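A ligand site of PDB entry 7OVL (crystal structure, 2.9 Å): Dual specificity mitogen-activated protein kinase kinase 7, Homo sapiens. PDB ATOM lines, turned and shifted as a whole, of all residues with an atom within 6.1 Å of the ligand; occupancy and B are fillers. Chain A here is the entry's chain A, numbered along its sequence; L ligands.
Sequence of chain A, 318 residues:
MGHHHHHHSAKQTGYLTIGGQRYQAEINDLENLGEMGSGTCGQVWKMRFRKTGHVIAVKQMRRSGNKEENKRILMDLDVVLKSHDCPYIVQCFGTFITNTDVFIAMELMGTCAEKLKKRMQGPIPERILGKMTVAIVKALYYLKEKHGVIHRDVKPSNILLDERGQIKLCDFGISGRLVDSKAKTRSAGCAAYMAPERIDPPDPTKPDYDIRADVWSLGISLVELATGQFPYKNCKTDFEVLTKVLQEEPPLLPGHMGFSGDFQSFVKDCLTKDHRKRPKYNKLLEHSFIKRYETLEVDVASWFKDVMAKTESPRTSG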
ATOM      1  N   MET A  36       6.931  19.485   3.987  1.00  0.00           N
ATOM      2  CA  MET A  36       6.961  18.996   5.351  1.00  0.00           C
ATOM      3  C   MET A  36       5.850  19.659   6.140  1.00  0.00           C
ATOM      4  O   MET A  36       5.228  20.623   5.698  1.00  0.00           O
ATOM      5  CB  MET A  36       8.317  19.252   6.014  1.00  0.00           C
ATOM      6  CG  MET A  36       8.585  20.723   6.280  1.00  0.00           C
ATOM      7  SD  MET A  36      10.174  21.016   7.073  1.00  0.00           S
ATOM      8  CE  MET A  36       9.954  22.694   7.638  1.00  0.00           C
ATOM      9  N   GLY A  37       5.596  19.126   7.337  1.00  0.00           N
ATOM     10  CA  GLY A  37       4.571  19.670   8.211  1.00  0.00           C
ATOM     11  C   GLY A  37       3.154  19.311   7.788  1.00  0.00           C
ATOM     12  O   GLY A  37       2.943  18.754   6.707  1.00  0.00           O
ATOM     13  N   VAL A  44       4.748  24.993   3.743  1.00  0.00           N
ATOM     14  CA  VAL A  44       6.110  25.187   4.237  1.00  0.00           C
ATOM     15  C   VAL A  44       6.993  24.091   3.640  1.00  0.00           C
ATOM     16  O   VAL A  44       6.647  22.906   3.700  1.00  0.00           O
ATOM     17  CB  VAL A  44       6.164  25.180   5.767  1.00  0.00           C
ATOM     18  CG1 VAL A  44       5.405  23.995   6.344  1.00  0.00           C
ATOM     19  CG2 VAL A  44       7.607  25.196   6.250  1.00  0.00           C
ATOM     20  N   LYS A  46      10.928  22.260   3.160  1.00  0.00           N
ATOM     21  CA  LYS A  46      12.277  22.045   3.642  1.00  0.00           C
ATOM     22  C   LYS A  46      13.225  22.308   2.470  1.00  0.00           C
ATOM     23  O   LYS A  46      13.253  21.541   1.506  1.00  0.00           O
ATOM     24  CB  LYS A  46      12.452  20.631   4.181  1.00  0.00           C
ATOM     25  CG  LYS A  46      13.890  20.246   4.518  1.00  0.00           C
ATOM     26  CD  LYS A  46      13.981  18.811   4.994  1.00  0.00           C
ATOM     27  CE  LYS A  46      15.429  18.375   5.175  1.00  0.00           C
ATOM     28  NZ  LYS A  46      15.541  16.974   5.654  1.00  0.00           N
ATOM     29  N   VAL A  55      20.337  23.684   5.566  1.00  0.00           N
ATOM     30  CA  VAL A  55      18.967  23.237   5.309  1.00  0.00           C
ATOM     31  C   VAL A  55      18.043  24.075   6.190  1.00  0.00           C
ATOM     32  O   VAL A  55      18.176  24.077   7.420  1.00  0.00           O
ATOM     33  CB  VAL A  55      18.804  21.737   5.577  1.00  0.00           C
ATOM     34  CG1 VAL A  55      19.564  21.324   6.835  1.00  0.00           C
ATOM     35  CG2 VAL A  55      17.331  21.381   5.708  1.00  0.00           C
ATOM     36  N   ALA A  57      13.894  26.084   6.635  1.00  0.00           N
ATOM     37  CA  ALA A  57      12.456  25.974   6.424  1.00  0.00           C
ATOM     38  C   ALA A  57      11.973  27.212   5.696  1.00  0.00           C
ATOM     39  O   ALA A  57      12.218  28.343   6.145  1.00  0.00           O
ATOM     40  CB  ALA A  57      11.718  25.814   7.757  1.00  0.00           C
ATOM     41  N   VAL A  90      10.907  30.769  17.034  1.00  0.00           N
ATOM     42  CA  VAL A  90      11.576  30.429  15.785  1.00  0.00           C
ATOM     43  C   VAL A  90      11.964  31.712  15.053  1.00  0.00           C
ATOM     44  O   VAL A  90      11.149  32.621  14.886  1.00  0.00           O
ATOM     45  CB  VAL A  90      10.691  29.526  14.916  1.00  0.00           C
ATOM     46  CG1 VAL A  90      10.583  28.142  15.535  1.00  0.00           C
ATOM     47  CG2 VAL A  90       9.310  30.133  14.739  1.00  0.00           C
ATOM     48  N   MET A 106      12.407  30.451   7.580  1.00  0.00           N
ATOM     49  CA  MET A 106      12.447  30.124   8.992  1.00  0.00           C
ATOM     50  C   MET A 106      13.532  29.100   9.270  1.00  0.00           C
ATOM     51  O   MET A 106      13.959  28.354   8.374  1.00  0.00           O
ATOM     52  CB  MET A 106      11.096  29.595   9.468  1.00  0.00           C
ATOM     53  CG  MET A 106       9.944  30.587   9.364  1.00  0.00           C
ATOM     54  SD  MET A 106      10.116  31.972  10.498  1.00  0.00           S
ATOM     55  CE  MET A 106       8.549  32.812  10.246  1.00  0.00           C
ATOM     56  N   GLU A 107      13.988  29.054  10.521  1.00  0.00           N
ATOM     57  CA  GLU A 107      14.984  28.070  10.905  1.00  0.00           C
ATOM     58  C   GLU A 107      14.348  26.679  10.973  1.00  0.00           C
ATOM     59  O   GLU A 107      13.150  26.526  11.213  1.00  0.00           O
ATOM     60  CB  GLU A 107      15.612  28.423  12.246  1.00  0.00           C
ATOM     61  CG  GLU A 107      14.659  28.377  13.433  1.00  0.00           C
ATOM     62  CD  GLU A 107      15.391  28.529  14.758  1.00  0.00           C
ATOM     63  OE1 GLU A 107      16.606  28.241  14.810  1.00  0.00           O
ATOM     64  OE2 GLU A 107      14.749  28.946  15.738  1.00  0.00           O
ATOM     65  N   LEU A 108      15.179  25.664  10.739  1.00  0.00           N
ATOM     66  CA  LEU A 108      14.711  24.294  10.677  1.00  0.00           C
ATOM     67  C   LEU A 108      14.791  23.645  12.049  1.00  0.00           C
ATOM     68  O   LEU A 108      15.820  23.733  12.725  1.00  0.00           O
ATOM     69  CB  LEU A 108      15.534  23.501   9.661  1.00  0.00           C
ATOM     70  CG  LEU A 108      14.892  22.280   8.997  1.00  0.00           C
ATOM     71  CD1 LEU A 108      14.885  21.076   9.936  1.00  0.00           C
ATOM     72  CD2 LEU A 108      13.478  22.602   8.541  1.00  0.00           C
ATOM     73  N   MET A 109      13.715  22.994  12.453  1.00  0.00           N
ATOM     74  CA  MET A 109      13.613  22.290  13.724  1.00  0.00           C
ATOM     75  C   MET A 109      13.263  20.831  13.462  1.00  0.00           C
ATOM     76  O   MET A 109      12.838  20.453  12.368  1.00  0.00           O
ATOM     77  CB  MET A 109      12.551  22.930  14.633  1.00  0.00           C
ATOM     78  CG  MET A 109      12.769  24.420  14.891  1.00  0.00           C
ATOM     79  SD  MET A 109      13.957  24.756  16.200  1.00  0.00           S
ATOM     80  CE  MET A 109      13.046  24.213  17.640  1.00  0.00           C
ATOM     81  N   GLY A 110      13.444  19.997  14.487  1.00  0.00           N
ATOM     82  CA  GLY A 110      13.179  18.578  14.371  1.00  0.00           C
ATOM     83  C   GLY A 110      11.719  18.261  14.115  1.00  0.00           C
ATOM     84  O   GLY A 110      11.364  17.762  13.043  1.00  0.00           O
ATOM     85  N   THR A 111      10.864  18.536  15.093  1.00  0.00           N
ATOM     86  CA  THR A 111       9.427  18.279  14.981  1.00  0.00           C
ATOM     87  C   THR A 111       8.707  19.088  16.050  1.00  0.00           C
ATOM     88  O   THR A 111       9.326  19.849  16.803  1.00  0.00           O
ATOM     89  CB  THR A 111       9.126  16.776  15.112  1.00  0.00           C
ATOM     90  OG1 THR A 111       7.732  16.551  14.881  1.00  0.00           O
ATOM     91  CG2 THR A 111       9.488  16.287  16.510  1.00  0.00           C
ATOM     92  N   CYS A 112       7.396  18.918  16.117  1.00  0.00           N
ATOM     93  CA  CYS A 112       6.570  19.600  17.111  1.00  0.00           C
ATOM     94  C   CYS A 112       6.294  18.681  18.295  1.00  0.00           C
ATOM     95  O   CYS A 112       6.612  17.485  18.282  1.00  0.00           O
ATOM     96  CB  CYS A 112       5.253  20.080  16.496  1.00  0.00           C
ATOM     97  SG  CYS A 112       4.174  18.771  15.871  1.00  0.00           S
ATOM     98  N   ALA A 113       5.683  19.255  19.336  1.00  0.00           N
ATOM     99  CA  ALA A 113       5.336  18.474  20.514  1.00  0.00           C
ATOM    100  C   ALA A 113       4.174  17.529  20.252  1.00  0.00           C
ATOM    101  O   ALA A 113       4.110  16.451  20.849  1.00  0.00           O
ATOM    102  CB  ALA A 113       5.021  19.400  21.680  1.00  0.00           C
ATOM    103  N   GLU A 114       3.260  17.913  19.352  1.00  0.00           N
ATOM    104  CA  GLU A 114       2.146  17.025  19.009  1.00  0.00           C
ATOM    105  C   GLU A 114       2.643  15.779  18.298  1.00  0.00           C
ATOM    106  O   GLU A 114       2.171  14.667  18.590  1.00  0.00           O
ATOM    107  CB  GLU A 114       1.127  17.768  18.142  1.00  0.00           C
ATOM    108  CG  GLU A 114      -0.064  16.923  17.743  1.00  0.00           C
ATOM    109  CD  GLU A 114      -0.926  17.593  16.687  1.00  0.00           C
ATOM    110  OE1 GLU A 114      -0.420  18.497  15.989  1.00  0.00           O
ATOM    111  OE2 GLU A 114      -2.112  17.215  16.558  1.00  0.00           O
ATOM    112  N   LYS A 115       3.587  15.926  17.372  1.00  0.00           N
ATOM    113  CA  LYS A 115       4.132  14.773  16.683  1.00  0.00           C
ATOM    114  C   LYS A 115       5.009  13.936  17.601  1.00  0.00           C
ATOM    115  O   LYS A 115       5.141  12.725  17.400  1.00  0.00           O
ATOM    116  CB  LYS A 115       4.924  15.211  15.449  1.00  0.00           C
ATOM    117  N   PRO A 156       0.232  21.746  21.683  1.00  0.00           N
ATOM    118  CA  PRO A 156       1.466  21.024  21.298  1.00  0.00           C
ATOM    119  C   PRO A 156       1.880  21.213  19.859  1.00  0.00           C
ATOM    120  O   PRO A 156       3.058  21.014  19.538  1.00  0.00           O
ATOM    121  CB  PRO A 156       1.109  19.563  21.600  1.00  0.00           C
ATOM    122  CG  PRO A 156       0.106  19.640  22.678  1.00  0.00           C
ATOM    123  CD  PRO A 156      -0.706  20.874  22.410  1.00  0.00           C
ATOM    124  N   SER A 157       0.963  21.601  18.972  1.00  0.00           N
ATOM    125  CA  SER A 157       1.298  21.798  17.569  1.00  0.00           C
ATOM    126  C   SER A 157       2.281  22.951  17.384  1.00  0.00           C
ATOM    127  O   SER A 157       3.047  22.961  16.409  1.00  0.00           O
ATOM    128  CB  SER A 157       0.041  22.048  16.744  1.00  0.00           C
ATOM    129  OG  SER A 157      -0.961  21.092  17.043  1.00  0.00           O
ATOM    130  N   ASN A 158       2.263  23.929  18.287  1.00  0.00           N
ATOM    131  CA  ASN A 158       3.077  25.126  18.163  1.00  0.00           C
ATOM    132  C   ASN A 158       4.309  25.090  19.066  1.00  0.00           C
ATOM    133  O   ASN A 158       4.920  26.139  19.317  1.00  0.00           O
ATOM    134  CB  ASN A 158       2.241  26.377  18.474  1.00  0.00           C
ATOM    135  CG  ASN A 158       1.077  26.539  17.527  1.00  0.00           C
ATOM    136  OD1 ASN A 158       0.011  25.958  17.713  1.00  0.00           O
ATOM    137  ND2 ASN A 158       1.271  27.340  16.485  1.00  0.00           N
ATOM    138  N   ILE A 159       4.692  23.915  19.551  1.00  0.00           N
ATOM    139  CA  ILE A 159       5.867  23.747  20.390  1.00  0.00           C
ATOM    140  C   ILE A 159       6.863  22.903  19.613  1.00  0.00           C
ATOM    141  O   ILE A 159       6.722  21.674  19.529  1.00  0.00           O
ATOM    142  CB  ILE A 159       5.512  23.115  21.743  1.00  0.00           C
ATOM    143  CG1 ILE A 159       4.456  23.943  22.460  1.00  0.00           C
ATOM    144  CG2 ILE A 159       6.756  22.965  22.605  1.00  0.00           C
ATOM    145  CD1 ILE A 159       4.001  23.350  23.777  1.00  0.00           C
ATOM    146  N   LEU A 160       7.874  23.547  19.042  1.00  0.00           N
ATOM    147  CA  LEU A 160       8.856  22.894  18.197  1.00  0.00           C
ATOM    148  C   LEU A 160      10.104  22.525  18.999  1.00  0.00           C
ATOM    149  O   LEU A 160      10.462  23.196  19.965  1.00  0.00           O
ATOM    150  CB  LEU A 160       9.250  23.768  17.017  1.00  0.00           C
ATOM    151  CG  LEU A 160       8.111  24.274  16.124  1.00  0.00           C
ATOM    152  CD1 LEU A 160       8.668  25.015  14.913  1.00  0.00           C
ATOM    153  CD2 LEU A 160       7.218  23.121  15.685  1.00  0.00           C
ATOM    154  N   GLU A 163      17.194  18.564  17.406  1.00  0.00           N
ATOM    155  CA  GLU A 163      18.185  17.638  17.923  1.00  0.00           C
ATOM    156  C   GLU A 163      19.230  18.315  18.801  1.00  0.00           C
ATOM    157  O   GLU A 163      20.085  17.625  19.370  1.00  0.00           O
ATOM    158  CB  GLU A 163      18.880  16.889  16.781  1.00  0.00           C
ATOM    159  CG  GLU A 163      19.782  17.771  15.925  1.00  0.00           C
ATOM    160  CD  GLU A 163      20.613  16.973  14.949  1.00  0.00           C
ATOM    161  OE1 GLU A 163      20.398  15.745  14.851  1.00  0.00           O
ATOM    162  OE2 GLU A 163      21.490  17.572  14.284  1.00  0.00           O
ATOM    163  N   CYS A 170       6.053  28.623  17.702  1.00  0.00           N
ATOM    164  CA  CYS A 170       5.868  28.584  16.257  1.00  0.00           C
ATOM    165  C   CYS A 170       4.661  29.423  15.857  1.00  0.00           C
ATOM    166  O   CYS A 170       3.602  29.322  16.496  1.00  0.00           O
ATOM    167  CB  CYS A 170       5.701  27.150  15.769  1.00  0.00           C
ATOM    168  SG  CYS A 170       5.262  26.984  14.027  1.00  0.00           S
ATOM    169  N   ASP A 171       4.835  30.229  14.802  1.00  0.00           N
ATOM    170  CA  ASP A 171       3.862  31.112  14.152  1.00  0.00           C
ATOM    171  C   ASP A 171       2.462  31.188  14.761  1.00  0.00           C
ATOM    172  O   ASP A 171       1.745  30.187  14.850  1.00  0.00           O
ATOM    173  CB  ASP A 171       3.740  30.729  12.684  1.00  0.00           C
ATOM    174  CG  ASP A 171       4.955  31.112  11.880  1.00  0.00           C
ATOM    175  OD1 ASP A 171       6.017  31.401  12.493  1.00  0.00           O
ATOM    176  OD2 ASP A 171       4.876  31.140  10.637  1.00  0.00           O
HETATM  177  C1  LIG L   1       9.964  20.714  10.701  1.00  0.00           C
HETATM  178  C2  LIG L   1       9.446  19.427  10.539  1.00  0.00           C
HETATM  179  C3  LIG L   1       8.102  19.182  10.821  1.00  0.00           C
HETATM  180  C4  LIG L   1       7.279  20.208  11.269  1.00  0.00           C
HETATM  181  C5  LIG L   1       7.809  21.482  11.421  1.00  0.00           C
HETATM  182  C6  LIG L   1       9.138  21.756  11.144  1.00  0.00           C
HETATM  183  C7  LIG L   1       9.660  22.983  11.307  1.00  0.00           C
HETATM  184  C8  LIG L   1       5.482  20.295  12.731  1.00  0.00           C
HETATM  185  C9  LIG L   1       4.005  19.948  12.911  1.00  0.00           C
HETATM  186  C10 LIG L   1       3.714  19.756  14.411  1.00  0.00           C
HETATM  187  C11 LIG L   1      10.196  18.347  10.092  1.00  0.00           C
HETATM  188  C12 LIG L   1      12.313  17.419   9.370  1.00  0.00           C
HETATM  189  C13 LIG L   1      13.820  17.672   9.407  1.00  0.00           C
HETATM  190  C14 LIG L   1      14.607  17.424  10.447  1.00  0.00           C
HETATM  191  C15 LIG L   1       9.988  25.104  11.506  1.00  0.00           C
HETATM  192  C16 LIG L   1       9.043  24.175  11.295  1.00  0.00           C
HETATM  193  C17 LIG L   1       9.696  26.402  11.542  1.00  0.00           C
HETATM  194  C18 LIG L   1       8.398  26.844  11.358  1.00  0.00           C
HETATM  195  C19 LIG L   1       7.411  25.898  11.136  1.00  0.00           C
HETATM  196  C20 LIG L   1       7.775  24.558  11.103  1.00  0.00           C
HETATM  197  C21 LIG L   1      17.007  17.621  11.047  1.00  0.00           C
HETATM  198  C22 LIG L   1      17.834  16.367  10.750  1.00  0.00           C
HETATM  199  C23 LIG L   1      18.541  16.515   9.414  1.00  0.00           C
HETATM  200  C24 LIG L   1      19.488  17.710   9.472  1.00  0.00           C
HETATM  201  C25 LIG L   1      18.687  18.979   9.741  1.00  0.00           C
HETATM  202  C26 LIG L   1      17.933  18.847  11.055  1.00  0.00           C
HETATM  203  C27 LIG L   1      19.347  14.855  11.723  1.00  0.00           C
HETATM  204  N1  LIG L   1       5.996  19.943  11.531  1.00  0.00           N
HETATM  205  N2  LIG L   1      11.507  18.544   9.854  1.00  0.00           N
HETATM  206  N3  LIG L   1      15.852  17.760  10.100  1.00  0.00           N
HETATM  207  N4  LIG L   1      15.807  18.188   8.824  1.00  0.00           N
HETATM  208  N5  LIG L   1      14.544  18.126   8.387  1.00  0.00           N
HETATM  209  N6  LIG L   1      10.949  23.157  11.532  1.00  0.00           N
HETATM  210  N7  LIG L   1      11.152  24.481  11.654  1.00  0.00           N
HETATM  211  O1  LIG L   1       6.102  20.844  13.631  1.00  0.00           O
HETATM  212  O2  LIG L   1       9.659  17.259   9.911  1.00  0.00           O
HETATM  213  O3  LIG L   1      18.807  16.175  11.788  1.00  0.00           O
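The backbone NH of Cys 112 lies close to an oxygen (O1) of the ligand.
SG of Cys 112 is bonded to C10 of the ligand (1.8 Å).
N7 of the ligand sits close to O of Glu 107, at 2.9 Å.
N of Met 109 is in hydrogen-bond range of N7 of the ligand, 3.1 Å away.
The backbone carbonyl oxygen (O) of Met 109 sits close to a nitrogen (N6) of the ligand (3.4 Å).
The side-chain amino group (NZ) of Lys 46 sits at hydrogen-bond distance from a nitrogen (N5) of the ligand.
A nitrogen (N2) of the ligand sits close to the backbone carbonyl oxygen (O) of Gly 110 (3.3 Å).
The side-chain sulfur (SG) of Cys 112 lies close to the backbone NH (N) of Glu 114, 3.7 Å away.
SG of Cys 112 lies within hydrogen-bond range of N of Lys 115, at 3.3 Å.
The backbone NH (N) of Met 36 lies within hydrogen-bond range of the backbone carbonyl oxygen (O) of Val 44 (3.4 Å).
The backbone carbonyl oxygen (O) of Cys 170 is in hydrogen-bond range of the side-chain amide nitrogen (ND2) of Asn 158 (3.1 Å).
The side-chain carboxylate (OE1) of Glu 114 sits at hydrogen-bond distance from the side-chain hydroxyl (OG) of Ser 157, at 2.9 Å.
The side-chain carboxylate (OE1) of Glu 163 lies close to an oxygen (O3) of the ligand.
Merely in contact with the ligand: Leu 108, Leu 160, Gly 37, Met 36, Cys 170, Ser 157, Val 55 and Thr 111.
Hydrophobic or aromatic side chains within 4 Å of the ligand: Met 36, Val 55, Leu 108, Met 109 and Leu 160.
Within 4 Å of the ligand: Met 36, Gly 37, Lys 46, Val 55, Glu 107, Leu 108, Met 109, Gly 110, Thr 111, Cys 112, Ser 157, Leu 160, Glu 163 and Cys 170.
Along chain A the residues within 4 Å of the ligand span positions 36 to 170.
The nearest printed residue that does not touch the ligand is Met 106 (4.1 Å).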
